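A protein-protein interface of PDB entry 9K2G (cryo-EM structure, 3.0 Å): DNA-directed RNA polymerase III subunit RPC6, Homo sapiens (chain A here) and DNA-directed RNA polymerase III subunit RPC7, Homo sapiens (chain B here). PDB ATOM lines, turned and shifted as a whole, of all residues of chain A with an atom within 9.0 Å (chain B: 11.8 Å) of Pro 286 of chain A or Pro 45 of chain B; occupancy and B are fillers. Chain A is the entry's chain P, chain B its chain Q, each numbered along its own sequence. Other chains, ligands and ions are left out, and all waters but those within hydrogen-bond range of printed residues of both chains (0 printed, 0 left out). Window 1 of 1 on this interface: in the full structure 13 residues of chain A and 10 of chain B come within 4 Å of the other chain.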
ATOM      1  N   PRO A 279      26.055  20.172   7.513  1.00  0.00           N
ATOM      2  CA  PRO A 279      25.593  21.182   6.550  1.00  0.00           C
ATOM      3  C   PRO A 279      25.466  22.549   7.206  1.00  0.00           C
ATOM      4  O   PRO A 279      25.034  22.673   8.353  1.00  0.00           O
ATOM      5  CB  PRO A 279      24.231  20.645   6.097  1.00  0.00           C
ATOM      6  CG  PRO A 279      24.357  19.172   6.257  1.00  0.00           C
ATOM      7  CD  PRO A 279      25.215  18.961   7.476  1.00  0.00           C
ATOM      8  N   THR A 280      25.857  23.579   6.461  1.00  0.00           N
ATOM      9  CA  THR A 280      25.921  24.925   7.002  1.00  0.00           C
ATOM     10  C   THR A 280      24.513  25.478   7.239  1.00  0.00           C
ATOM     11  O   THR A 280      23.512  24.929   6.775  1.00  0.00           O
ATOM     12  CB  THR A 280      26.705  25.846   6.066  1.00  0.00           C
ATOM     13  OG1 THR A 280      25.995  25.982   4.826  1.00  0.00           O
ATOM     14  CG2 THR A 280      28.076  25.263   5.791  1.00  0.00           C
ATOM     15  N   GLY A 281      24.455  26.582   7.981  1.00  0.00           N
ATOM     16  CA  GLY A 281      23.174  27.196   8.279  1.00  0.00           C
ATOM     17  C   GLY A 281      22.516  27.829   7.069  1.00  0.00           C
ATOM     18  O   GLY A 281      21.291  27.971   7.028  1.00  0.00           O
ATOM     19  N   LEU A 282      23.312  28.208   6.062  1.00  0.00           N
ATOM     20  CA  LEU A 282      22.761  28.872   4.883  1.00  0.00           C
ATOM     21  C   LEU A 282      21.791  27.969   4.137  1.00  0.00           C
ATOM     22  O   LEU A 282      20.718  28.412   3.711  1.00  0.00           O
ATOM     23  CB  LEU A 282      23.888  29.324   3.959  1.00  0.00           C
ATOM     24  CG  LEU A 282      23.449  29.837   2.586  1.00  0.00           C
ATOM     25  CD1 LEU A 282      22.573  31.078   2.720  1.00  0.00           C
ATOM     26  CD2 LEU A 282      24.654  30.110   1.699  1.00  0.00           C
ATOM     27  N   VAL A 283      22.148  26.693   3.959  1.00  0.00           N
ATOM     28  CA  VAL A 283      21.286  25.766   3.232  1.00  0.00           C
ATOM     29  C   VAL A 283      20.057  25.363   4.026  1.00  0.00           C
ATOM     30  O   VAL A 283      19.151  24.736   3.467  1.00  0.00           O
ATOM     31  CB  VAL A 283      22.064  24.509   2.808  1.00  0.00           C
ATOM     32  CG1 VAL A 283      23.275  24.896   1.980  1.00  0.00           C
ATOM     33  CG2 VAL A 283      22.477  23.702   4.027  1.00  0.00           C
ATOM     34  N   ARG A 284      20.001  25.699   5.315  1.00  0.00           N
ATOM     35  CA  ARG A 284      18.825  25.410   6.124  1.00  0.00           C
ATOM     36  C   ARG A 284      17.712  26.435   5.934  1.00  0.00           C
ATOM     37  O   ARG A 284      16.623  26.251   6.487  1.00  0.00           O
ATOM     38  CB  ARG A 284      19.211  25.323   7.600  1.00  0.00           C
ATOM     39  CG  ARG A 284      20.106  24.140   7.923  1.00  0.00           C
ATOM     40  CD  ARG A 284      20.343  23.996   9.415  1.00  0.00           C
ATOM     41  NE  ARG A 284      20.974  22.726   9.738  1.00  0.00           N
ATOM     42  CZ  ARG A 284      22.284  22.523   9.750  1.00  0.00           C
ATOM     43  NH1 ARG A 284      23.140  23.493   9.470  1.00  0.00           N
ATOM     44  NH2 ARG A 284      22.753  21.314  10.054  1.00  0.00           N
ATOM     45  N   ALA A 285      17.961  27.498   5.167  1.00  0.00           N
ATOM     46  CA  ALA A 285      16.956  28.489   4.826  1.00  0.00           C
ATOM     47  C   ALA A 285      16.612  28.401   3.343  1.00  0.00           C
ATOM     48  O   ALA A 285      17.493  28.127   2.522  1.00  0.00           O
ATOM     49  CB  ALA A 285      17.440  29.907   5.149  1.00  0.00           C
ATOM     50  N   PRO A 286      15.343  28.606   2.973  1.00  0.00           N
ATOM     51  CA  PRO A 286      14.972  28.512   1.552  1.00  0.00           C
ATOM     52  C   PRO A 286      15.705  29.497   0.661  1.00  0.00           C
ATOM     53  O   PRO A 286      15.975  29.181  -0.502  1.00  0.00           O
ATOM     54  CB  PRO A 286      13.462  28.786   1.569  1.00  0.00           C
ATOM     55  CG  PRO A 286      13.028  28.484   2.964  1.00  0.00           C
ATOM     56  CD  PRO A 286      14.183  28.880   3.834  1.00  0.00           C
ATOM     57  N   CYS A 287      16.029  30.689   1.171  1.00  0.00           N
ATOM     58  CA  CYS A 287      16.730  31.679   0.359  1.00  0.00           C
ATOM     59  C   CYS A 287      18.117  31.196  -0.048  1.00  0.00           C
ATOM     60  O   CYS A 287      18.638  31.616  -1.087  1.00  0.00           O
ATOM     61  CB  CYS A 287      16.827  33.002   1.116  1.00  0.00           C
ATOM     62  SG  CYS A 287      15.231  33.672   1.633  1.00  0.00           S
ATOM     63  N   GLY A 288      18.725  30.318   0.753  1.00  0.00           N
ATOM     64  CA  GLY A 288      20.010  29.753   0.390  1.00  0.00           C
ATOM     65  C   GLY A 288      19.945  28.764  -0.751  1.00  0.00           C
ATOM     66  O   GLY A 288      20.964  28.518  -1.403  1.00  0.00           O
ATOM     67  N   LEU A 289      18.771  28.190  -1.010  1.00  0.00           N
ATOM     68  CA  LEU A 289      18.578  27.244  -2.100  1.00  0.00           C
ATOM     69  C   LEU A 289      17.632  27.767  -3.176  1.00  0.00           C
ATOM     70  O   LEU A 289      17.289  27.019  -4.101  1.00  0.00           O
ATOM     71  CB  LEU A 289      18.053  25.911  -1.561  1.00  0.00           C
ATOM     72  CG  LEU A 289      18.848  25.266  -0.420  1.00  0.00           C
ATOM     73  CD1 LEU A 289      18.277  23.904  -0.073  1.00  0.00           C
ATOM     74  CD2 LEU A 289      20.327  25.164  -0.769  1.00  0.00           C
ATOM     75  N   CYS A 290      17.202  29.017  -3.078  1.00  0.00           N
ATOM     76  CA  CYS A 290      16.245  29.553  -4.036  1.00  0.00           C
ATOM     77  C   CYS A 290      16.884  29.684  -5.417  1.00  0.00           C
ATOM     78  O   CYS A 290      17.974  30.257  -5.536  1.00  0.00           O
ATOM     79  CB  CYS A 290      15.729  30.911  -3.575  1.00  0.00           C
ATOM     80  SG  CYS A 290      14.784  31.781  -4.840  1.00  0.00           S
ATOM     81  N   PRO A 291      16.244  29.172  -6.470  1.00  0.00           N
ATOM     82  CA  PRO A 291      16.815  29.319  -7.817  1.00  0.00           C
ATOM     83  C   PRO A 291      16.582  30.684  -8.439  1.00  0.00           C
ATOM     84  O   PRO A 291      17.264  31.019  -9.417  1.00  0.00           O
ATOM     85  CB  PRO A 291      16.095  28.227  -8.616  1.00  0.00           C
ATOM     86  CG  PRO A 291      14.757  28.138  -7.958  1.00  0.00           C
ATOM     87  CD  PRO A 291      14.982  28.407  -6.487  1.00  0.00           C
ATOM     88  N   VAL A 292      15.649  31.472  -7.909  1.00  0.00           N
ATOM     89  CA  VAL A 292      15.326  32.781  -8.471  1.00  0.00           C
ATOM     90  C   VAL A 292      15.760  33.846  -7.470  1.00  0.00           C
ATOM     91  O   VAL A 292      15.190  34.939  -7.401  1.00  0.00           O
ATOM     92  CB  VAL A 292      13.828  32.864  -8.833  1.00  0.00           C
ATOM     93  CG1 VAL A 292      12.930  32.951  -7.591  1.00  0.00           C
ATOM     94  CG2 VAL A 292      13.561  34.002  -9.821  1.00  0.00           C
ATOM     95  N   PHE A 293      16.808  33.528  -6.703  1.00  0.00           N
ATOM     96  CA  PHE A 293      17.312  34.433  -5.670  1.00  0.00           C
ATOM     97  C   PHE A 293      17.671  35.801  -6.239  1.00  0.00           C
ATOM     98  O   PHE A 293      17.507  36.826  -5.563  1.00  0.00           O
ATOM     99  CB  PHE A 293      18.528  33.797  -4.990  1.00  0.00           C
ATOM    100  CG  PHE A 293      19.311  34.741  -4.123  1.00  0.00           C
ATOM    101  CD1 PHE A 293      18.892  35.032  -2.832  1.00  0.00           C
ATOM    102  CD2 PHE A 293      20.481  35.322  -4.585  1.00  0.00           C
ATOM    103  CE1 PHE A 293      19.618  35.894  -2.031  1.00  0.00           C
ATOM    104  CE2 PHE A 293      21.205  36.187  -3.788  1.00  0.00           C
ATOM    105  CZ  PHE A 293      20.774  36.469  -2.510  1.00  0.00           C
ATOM    106  N   CYS A 307       6.553  34.776  -0.902  1.00  0.00           N
ATOM    107  CA  CYS A 307       7.386  33.722  -1.469  1.00  0.00           C
ATOM    108  C   CYS A 307       6.788  32.348  -1.186  1.00  0.00           C
ATOM    109  O   CYS A 307       6.390  32.049  -0.056  1.00  0.00           O
ATOM    110  CB  CYS A 307       8.801  33.808  -0.901  1.00  0.00           C
ATOM    111  SG  CYS A 307       9.910  32.530  -1.529  1.00  0.00           S
ATOM    112  N   ILE A 308       6.723  31.514  -2.223  1.00  0.00           N
ATOM    113  CA  ILE A 308       6.140  30.182  -2.089  1.00  0.00           C
ATOM    114  C   ILE A 308       7.066  29.258  -1.308  1.00  0.00           C
ATOM    115  O   ILE A 308       6.608  28.381  -0.561  1.00  0.00           O
ATOM    116  CB  ILE A 308       5.807  29.609  -3.483  1.00  0.00           C
ATOM    117  CG1 ILE A 308       4.751  30.476  -4.168  1.00  0.00           C
ATOM    118  CG2 ILE A 308       5.326  28.166  -3.389  1.00  0.00           C
ATOM    119  CD1 ILE A 308       3.450  30.577  -3.400  1.00  0.00           C
ATOM    120  N   TYR A 309       8.381  29.417  -1.480  1.00  0.00           N
ATOM    121  CA  TYR A 309       9.328  28.493  -0.867  1.00  0.00           C
ATOM    122  C   TYR A 309       9.217  28.517   0.653  1.00  0.00           C
ATOM    123  O   TYR A 309       9.139  27.465   1.295  1.00  0.00           O
ATOM    124  CB  TYR A 309      10.749  28.832  -1.315  1.00  0.00           C
ATOM    125  CG  TYR A 309      10.945  28.724  -2.808  1.00  0.00           C
ATOM    126  CD1 TYR A 309      11.140  27.492  -3.414  1.00  0.00           C
ATOM    127  CD2 TYR A 309      10.913  29.856  -3.612  1.00  0.00           C
ATOM    128  CE1 TYR A 309      11.309  27.390  -4.785  1.00  0.00           C
ATOM    129  CE2 TYR A 309      11.083  29.761  -4.982  1.00  0.00           C
ATOM    130  CZ  TYR A 309      11.279  28.527  -5.563  1.00  0.00           C
ATOM    131  OH  TYR A 309      11.445  28.431  -6.925  1.00  0.00           O
ATOM    132  N   MET A 310       9.182  29.714   1.239  1.00  0.00           N
ATOM    133  CA  MET A 310       9.004  29.805   2.682  1.00  0.00           C
ATOM    134  C   MET A 310       7.615  29.359   3.107  1.00  0.00           C
ATOM    135  O   MET A 310       7.453  28.830   4.211  1.00  0.00           O
ATOM    136  CB  MET A 310       9.288  31.226   3.158  1.00  0.00           C
ATOM    137  CG  MET A 310      10.663  31.393   3.777  1.00  0.00           C
ATOM    138  SD  MET A 310      11.310  33.049   3.518  1.00  0.00           S
ATOM    139  CE  MET A 310      11.298  33.105   1.729  1.00  0.00           C
ATOM    140  N   THR A 311       6.608  29.538   2.251  1.00  0.00           N
ATOM    141  CA  THR A 311       5.271  29.039   2.567  1.00  0.00           C
ATOM    142  C   THR A 311       5.280  27.523   2.745  1.00  0.00           C
ATOM    143  O   THR A 311       4.821  27.000   3.764  1.00  0.00           O
ATOM    144  CB  THR A 311       4.282  29.443   1.468  1.00  0.00           C
ATOM    145  OG1 THR A 311       4.333  30.863   1.272  1.00  0.00           O
ATOM    146  CG2 THR A 311       2.869  29.044   1.848  1.00  0.00           C
ATOM    147  N   GLU A 312       5.829  26.804   1.760  1.00  0.00           N
ATOM    148  CA  GLU A 312       5.928  25.351   1.868  1.00  0.00           C
ATOM    149  C   GLU A 312       6.828  24.944   3.030  1.00  0.00           C
ATOM    150  O   GLU A 312       6.527  23.984   3.751  1.00  0.00           O
ATOM    151  CB  GLU A 312       6.449  24.758   0.560  1.00  0.00           C
ATOM    152  CG  GLU A 312       5.525  24.942  -0.633  1.00  0.00           C
ATOM    153  CD  GLU A 312       6.102  24.357  -1.907  1.00  0.00           C
ATOM    154  OE1 GLU A 312       7.199  23.764  -1.844  1.00  0.00           O
ATOM    155  OE2 GLU A 312       5.461  24.489  -2.971  1.00  0.00           O
ATOM    156  N   TRP A 313       7.941  25.654   3.213  1.00  0.00           N
ATOM    157  CA  TRP A 313       8.906  25.289   4.248  1.00  0.00           C
ATOM    158  C   TRP A 313       8.323  25.446   5.646  1.00  0.00           C
ATOM    159  O   TRP A 313       8.532  24.591   6.516  1.00  0.00           O
ATOM    160  CB  TRP A 313      10.166  26.132   4.064  1.00  0.00           C
ATOM    161  CG  TRP A 313      11.195  25.974   5.123  1.00  0.00           C
ATOM    162  CD1 TRP A 313      11.859  24.832   5.462  1.00  0.00           C
ATOM    163  CD2 TRP A 313      11.722  27.009   5.954  1.00  0.00           C
ATOM    164  NE1 TRP A 313      12.754  25.088   6.473  1.00  0.00           N
ATOM    165  CE2 TRP A 313      12.687  26.420   6.791  1.00  0.00           C
ATOM    166  CE3 TRP A 313      11.462  28.376   6.083  1.00  0.00           C
ATOM    167  CZ2 TRP A 313      13.394  27.152   7.742  1.00  0.00           C
ATOM    168  CZ3 TRP A 313      12.163  29.099   7.022  1.00  0.00           C
ATOM    169  CH2 TRP A 313      13.116  28.486   7.838  1.00  0.00           C
ATOM    170  N   LEU A 314       7.586  26.535   5.890  1.00  0.00           N
ATOM    171  CA  LEU A 314       6.960  26.731   7.194  1.00  0.00           C
ATOM    172  C   LEU A 314       5.767  25.801   7.376  1.00  0.00           C
ATOM    173  O   LEU A 314       5.524  25.309   8.485  1.00  0.00           O
ATOM    174  CB  LEU A 314       6.534  28.190   7.363  1.00  0.00           C
ATOM    175  CG  LEU A 314       7.649  29.235   7.406  1.00  0.00           C
ATOM    176  CD1 LEU A 314       7.069  30.631   7.592  1.00  0.00           C
ATOM    177  CD2 LEU A 314       8.653  28.916   8.497  1.00  0.00           C
ATOM    178  N   PHE A 316       5.524  22.817   6.073  1.00  0.00           N
ATOM    179  CA  PHE A 316       6.161  21.534   6.355  1.00  0.00           C
ATOM    180  C   PHE A 316       6.836  21.571   7.721  1.00  0.00           C
ATOM    181  O   PHE A 316       7.099  22.641   8.268  1.00  0.00           O
ATOM    182  CB  PHE A 316       7.176  21.189   5.257  1.00  0.00           C
ATOM    183  CG  PHE A 316       7.960  19.937   5.528  1.00  0.00           C
ATOM    184  CD1 PHE A 316       9.220  20.000   6.101  1.00  0.00           C
ATOM    185  CD2 PHE A 316       7.440  18.695   5.205  1.00  0.00           C
ATOM    186  CE1 PHE A 316       9.943  18.853   6.348  1.00  0.00           C
ATOM    187  CE2 PHE A 316       8.162  17.538   5.450  1.00  0.00           C
ATOM    188  CZ  PHE A 316       9.414  17.618   6.022  1.00  0.00           C
ATOM    189  N   PHE B  38       7.483  30.982  -9.399  1.00  0.00           N
ATOM    190  CA  PHE B  38       8.356  30.257  -8.478  1.00  0.00           C
ATOM    191  C   PHE B  38       8.556  28.846  -9.021  1.00  0.00           C
ATOM    192  O   PHE B  38       7.763  27.942  -8.724  1.00  0.00           O
ATOM    193  CB  PHE B  38       7.764  30.222  -7.068  1.00  0.00           C
ATOM    194  CG  PHE B  38       7.592  31.580  -6.444  1.00  0.00           C
ATOM    195  CD1 PHE B  38       6.441  32.314  -6.668  1.00  0.00           C
ATOM    196  CD2 PHE B  38       8.576  32.113  -5.630  1.00  0.00           C
ATOM    197  CE1 PHE B  38       6.275  33.562  -6.095  1.00  0.00           C
ATOM    198  CE2 PHE B  38       8.418  33.358  -5.053  1.00  0.00           C
ATOM    199  CZ  PHE B  38       7.267  34.086  -5.288  1.00  0.00           C
ATOM    200  N   PRO B  39       9.586  28.621  -9.834  1.00  0.00           N
ATOM    201  CA  PRO B  39       9.848  27.262 -10.325  1.00  0.00           C
ATOM    202  C   PRO B  39      10.161  26.319  -9.174  1.00  0.00           C
ATOM    203  O   PRO B  39      10.832  26.689  -8.209  1.00  0.00           O
ATOM    204  CB  PRO B  39      11.052  27.448 -11.257  1.00  0.00           C
ATOM    205  CG  PRO B  39      11.707  28.707 -10.782  1.00  0.00           C
ATOM    206  CD  PRO B  39      10.592  29.588 -10.314  1.00  0.00           C
ATOM    207  N   ASP B  40       9.670  25.089  -9.285  1.00  0.00           N
ATOM    208  CA  ASP B  40       9.829  24.127  -8.205  1.00  0.00           C
ATOM    209  C   ASP B  40      11.263  23.608  -8.139  1.00  0.00           C
ATOM    210  O   ASP B  40      11.991  23.590  -9.132  1.00  0.00           O
ATOM    211  CB  ASP B  40       8.853  22.960  -8.369  1.00  0.00           C
ATOM    212  CG  ASP B  40       8.993  22.250  -9.705  1.00  0.00           C
ATOM    213  OD1 ASP B  40       9.774  22.718 -10.563  1.00  0.00           O
ATOM    214  OD2 ASP B  40       8.315  21.222  -9.904  1.00  0.00           O
ATOM    215  N   THR B  41      11.668  23.201  -6.941  1.00  0.00           N
ATOM    216  CA  THR B  41      12.986  22.638  -6.693  1.00  0.00           C
ATOM    217  C   THR B  41      12.835  21.281  -6.017  1.00  0.00           C
ATOM    218  O   THR B  41      12.037  21.130  -5.089  1.00  0.00           O
ATOM    219  CB  THR B  41      13.833  23.563  -5.816  1.00  0.00           C
ATOM    220  OG1 THR B  41      13.124  23.853  -4.609  1.00  0.00           O
ATOM    221  CG2 THR B  41      14.130  24.861  -6.546  1.00  0.00           C
ATOM    222  N   ASP B  42      13.604  20.303  -6.479  1.00  0.00           N
ATOM    223  CA  ASP B  42      13.562  18.967  -5.896  1.00  0.00           C
ATOM    224  C   ASP B  42      14.452  18.829  -4.668  1.00  0.00           C
ATOM    225  O   ASP B  42      14.479  17.756  -4.056  1.00  0.00           O
ATOM    226  CB  ASP B  42      13.939  17.906  -6.939  1.00  0.00           C
ATOM    227  CG  ASP B  42      15.366  18.046  -7.443  1.00  0.00           C
ATOM    228  OD1 ASP B  42      16.026  19.064  -7.141  1.00  0.00           O
ATOM    229  OD2 ASP B  42      15.822  17.125  -8.151  1.00  0.00           O
ATOM    230  N   TYR B  43      15.197  19.872  -4.310  1.00  0.00           N
ATOM    231  CA  TYR B  43      15.955  19.910  -3.068  1.00  0.00           C
ATOM    232  C   TYR B  43      15.261  20.840  -2.081  1.00  0.00           C
ATOM    233  O   TYR B  43      14.895  21.967  -2.427  1.00  0.00           O
ATOM    234  CB  TYR B  43      17.394  20.391  -3.306  1.00  0.00           C
ATOM    235  CG  TYR B  43      18.219  19.464  -4.170  1.00  0.00           C
ATOM    236  CD1 TYR B  43      18.707  18.266  -3.670  1.00  0.00           C
ATOM    237  CD2 TYR B  43      18.521  19.802  -5.483  1.00  0.00           C
ATOM    238  CE1 TYR B  43      19.464  17.420  -4.457  1.00  0.00           C
ATOM    239  CE2 TYR B  43      19.281  18.962  -6.275  1.00  0.00           C
ATOM    240  CZ  TYR B  43      19.750  17.772  -5.760  1.00  0.00           C
ATOM    241  OH  TYR B  43      20.503  16.942  -6.557  1.00  0.00           O
ATOM    242  N   LYS B  44      15.081  20.363  -0.857  1.00  0.00           N
ATOM    243  CA  LYS B  44      14.440  21.163   0.172  1.00  0.00           C
ATOM    244  C   LYS B  44      15.454  21.558   1.239  1.00  0.00           C
ATOM    245  O   LYS B  44      16.473  20.879   1.415  1.00  0.00           O
ATOM    246  CB  LYS B  44      13.275  20.404   0.821  1.00  0.00           C
ATOM    247  CG  LYS B  44      12.314  19.776  -0.181  1.00  0.00           C
ATOM    248  CD  LYS B  44      11.837  20.782  -1.229  1.00  0.00           C
ATOM    249  CE  LYS B  44      10.918  21.848  -0.641  1.00  0.00           C
ATOM    250  NZ  LYS B  44      10.435  22.793  -1.693  1.00  0.00           N
ATOM    251  N   PRO B  45      15.221  22.657   1.957  1.00  0.00           N
ATOM    252  CA  PRO B  45      16.178  23.085   2.982  1.00  0.00           C
ATOM    253  C   PRO B  45      16.376  22.024   4.053  1.00  0.00           C
ATOM    254  O   PRO B  45      15.447  21.312   4.434  1.00  0.00           O
ATOM    255  CB  PRO B  45      15.541  24.355   3.558  1.00  0.00           C
ATOM    256  CG  PRO B  45      14.674  24.867   2.458  1.00  0.00           C
ATOM    257  CD  PRO B  45      14.146  23.648   1.761  1.00  0.00           C
ATOM    258  N   VAL B  46      17.615  21.924   4.531  1.00  0.00           N
ATOM    259  CA  VAL B  46      17.947  20.956   5.585  1.00  0.00           C
ATOM    260  C   VAL B  46      17.192  21.325   6.854  1.00  0.00           C
ATOM    261  O   VAL B  46      17.084  22.523   7.185  1.00  0.00           O
ATOM    262  CB  VAL B  46      19.466  20.931   5.829  1.00  0.00           C
ATOM    263  CG1 VAL B  46      19.830  19.994   6.976  1.00  0.00           C
ATOM    264  CG2 VAL B  46      20.198  20.525   4.557  1.00  0.00           C
ATOM    265  N   PRO B  47      16.634  20.363   7.590  1.00  0.00           N
ATOM    266  CA  PRO B  47      15.944  20.700   8.844  1.00  0.00           C
ATOM    267  C   PRO B  47      16.882  21.380   9.834  1.00  0.00           C
ATOM    268  O   PRO B  47      18.078  21.091   9.891  1.00  0.00           O
ATOM    269  CB  PRO B  47      15.467  19.340   9.368  1.00  0.00           C
ATOM    270  CG  PRO B  47      16.259  18.319   8.608  1.00  0.00           C
ATOM    271  CD  PRO B  47      16.512  18.934   7.269  1.00  0.00           C
ATOM    272  N   LEU B  48      16.312  22.297  10.610  1.00  0.00           N
ATOM    273  CA  LEU B  48      17.092  23.121  11.519  1.00  0.00           C
ATOM    274  C   LEU B  48      17.712  22.283  12.633  1.00  0.00           C
ATOM    275  O   LEU B  48      17.176  21.246  13.036  1.00  0.00           O
ATOM    276  CB  LEU B  48      16.221  24.223  12.124  1.00  0.00           C
ATOM    277  CG  LEU B  48      16.012  25.505  11.313  1.00  0.00           C
ATOM    278  CD1 LEU B  48      17.347  26.156  10.995  1.00  0.00           C
ATOM    279  CD2 LEU B  48      15.226  25.237  10.037  1.00  0.00           C
ATOM    280  N   LYS B  49      18.856  22.747  13.125  1.00  0.00           N
ATOM    281  CA  LYS B  49      19.516  22.092  14.244  1.00  0.00           C
ATOM    282  C   LYS B  49      18.659  22.200  15.498  1.00  0.00           C
ATOM    283  O   LYS B  49      18.002  23.217  15.736  1.00  0.00           O
ATOM    284  CB  LYS B  49      20.891  22.705  14.486  1.00  0.00           C
ATOM    285  CG  LYS B  49      21.778  22.750  13.250  1.00  0.00           C
ATOM    286  CD  LYS B  49      23.137  23.347  13.572  1.00  0.00           C
ATOM    287  CE  LYS B  49      23.831  22.565  14.672  1.00  0.00           C
ATOM    288  NZ  LYS B  49      23.930  21.116  14.341  1.00  0.00           N
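Pro 286 of chain A touches just one residue of chain B: Pro 45.
Pro 45 of chain B touches four residues of chain A.
Val 283 of chain A touches two residues of chain B.
No residue of chain B comes within 4 Å of Ala 285 of chain A.
No residue of chain B comes within 4 Å of Cys 287 of chain A.
No residue of chain B comes within 4 Å of Gly 288 of chain A.
Of chain B, only Lys 44 (3.8 Å) and Pro 45 (3.8 Å) come within 4 Å of Leu 289 of chain A.
No residue of chain B comes within 4 Å of Cys 290 of chain A.
Met 310 of chain A touches none of the printed residues of chain B.
Printed residues of chain A within 4 Å of Val 46 of chain B: Val 283 and Arg 284.
Of the printed residues of chain B, Cys 307 of chain A touches Phe 38 (3.7 Å).
Printed residues of chain A within 4 Å of Leu 48 of chain B: Arg 284 (3.9 Å) and Trp 313 (3.5 Å).
Of the printed residues of chain B, Tyr 309 of chain A touches Phe 38 (3.5 Å), Pro 39 (2.2 Å) and Thr 41 (3.98 Å).
Of the printed residues of chain A, Thr 41 of chain B touches Pro 291 (3.6 Å) and Tyr 309 (3.98 Å).
Thr 311 of chain A touches none of the printed residues of chain B.
Phe 316 of chain A touches none of the printed residues of chain B.
The nearest residue of chain B that does not touch Pro 286 of chain A is Lys 44 of chain B (7.0 Å).
The nearest printed residue of chain B that does not touch Tyr 309 of chain A is Asp 40 of chain B (4.5 Å).
N of Val 46 of chain B sits at hydrogen-bond distance from O of Val 283 of chain A (3.4 Å).
The guanidinium group (NE) of Arg 284 of chain A sits at hydrogen-bond distance from the backbone carbonyl oxygen (O) of Pro 47 of chain B (3.3 Å).
The side-chain carboxylate (OE1) of Glu 312 of chain A is in salt-bridge range of the side-chain amino group (NZ) of Lys 44 of chain B (3.4 Å).
OH of Tyr 309 of chain A sits close to O of Pro 39 of chain B.
Among the printed residues, merely in contact across the chains: Val 283 of chain A with Pro 45 of chain B, Tyr 309 of chain A with Phe 38 of chain B, Trp 313 of chain A with Leu 48 of chain B, Arg 284 of chain A with Val 46 of chain B, Ile 308 of chain A with Phe 38 of chain B, Arg 284 of chain A with Lys 49 of chain B, Pro 291 of chain A with Thr 41 of chain B, Arg 284 of chain A with Pro 45 of chain B, Cys 307 of chain A with Phe 38 of chain B, Pro 286 of chain A with Pro 45 of chain B, Leu 289 of chain A with Pro 45 of chain B, Leu 289 of chain A with Lys 44 of chain B, Arg 284 of chain A with Leu 48 of chain B and Tyr 309 of chain A with Thr 41 of chain B.
Hydrophobic or aromatic side chains of chain A that line the printed part of chain B: Val 283, Leu 289, Pro 291, Ile 308, Tyr 309 and Trp 313.
Of the 12 printed residues of chain B, 9 touch a printed residue of chain A.
Among the printed residues, Asp or Glu carboxylates within 4 Å of a Lys or Arg side-chain nitrogen of the other chain: Glu 312 of chain A with Lys 44 of chain B.
The backbone carbonyl oxygen (O) of Pro 279 of chain A sits close to the guanidinium group (NH2) of Arg 284 of chain A, 3.2 Å away.
O of Thr 280 of chain A lies within hydrogen-bond range of NH1 of Arg 284 of chain A (3.1 Å).
SG of Cys 307 of chain A lies close to N of Tyr 309 of chain A.
The backbone carbonyl oxygen (O) of Cys 307 of chain A is in hydrogen-bond range of the side-chain hydroxyl (OG1) of Thr 311 of chain A.
The side-chain hydroxyl of Thr 41 of chain B is in hydrogen-bond range of the backbone carbonyl oxygen of Tyr 43 of chain B, 3.4 Å away.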
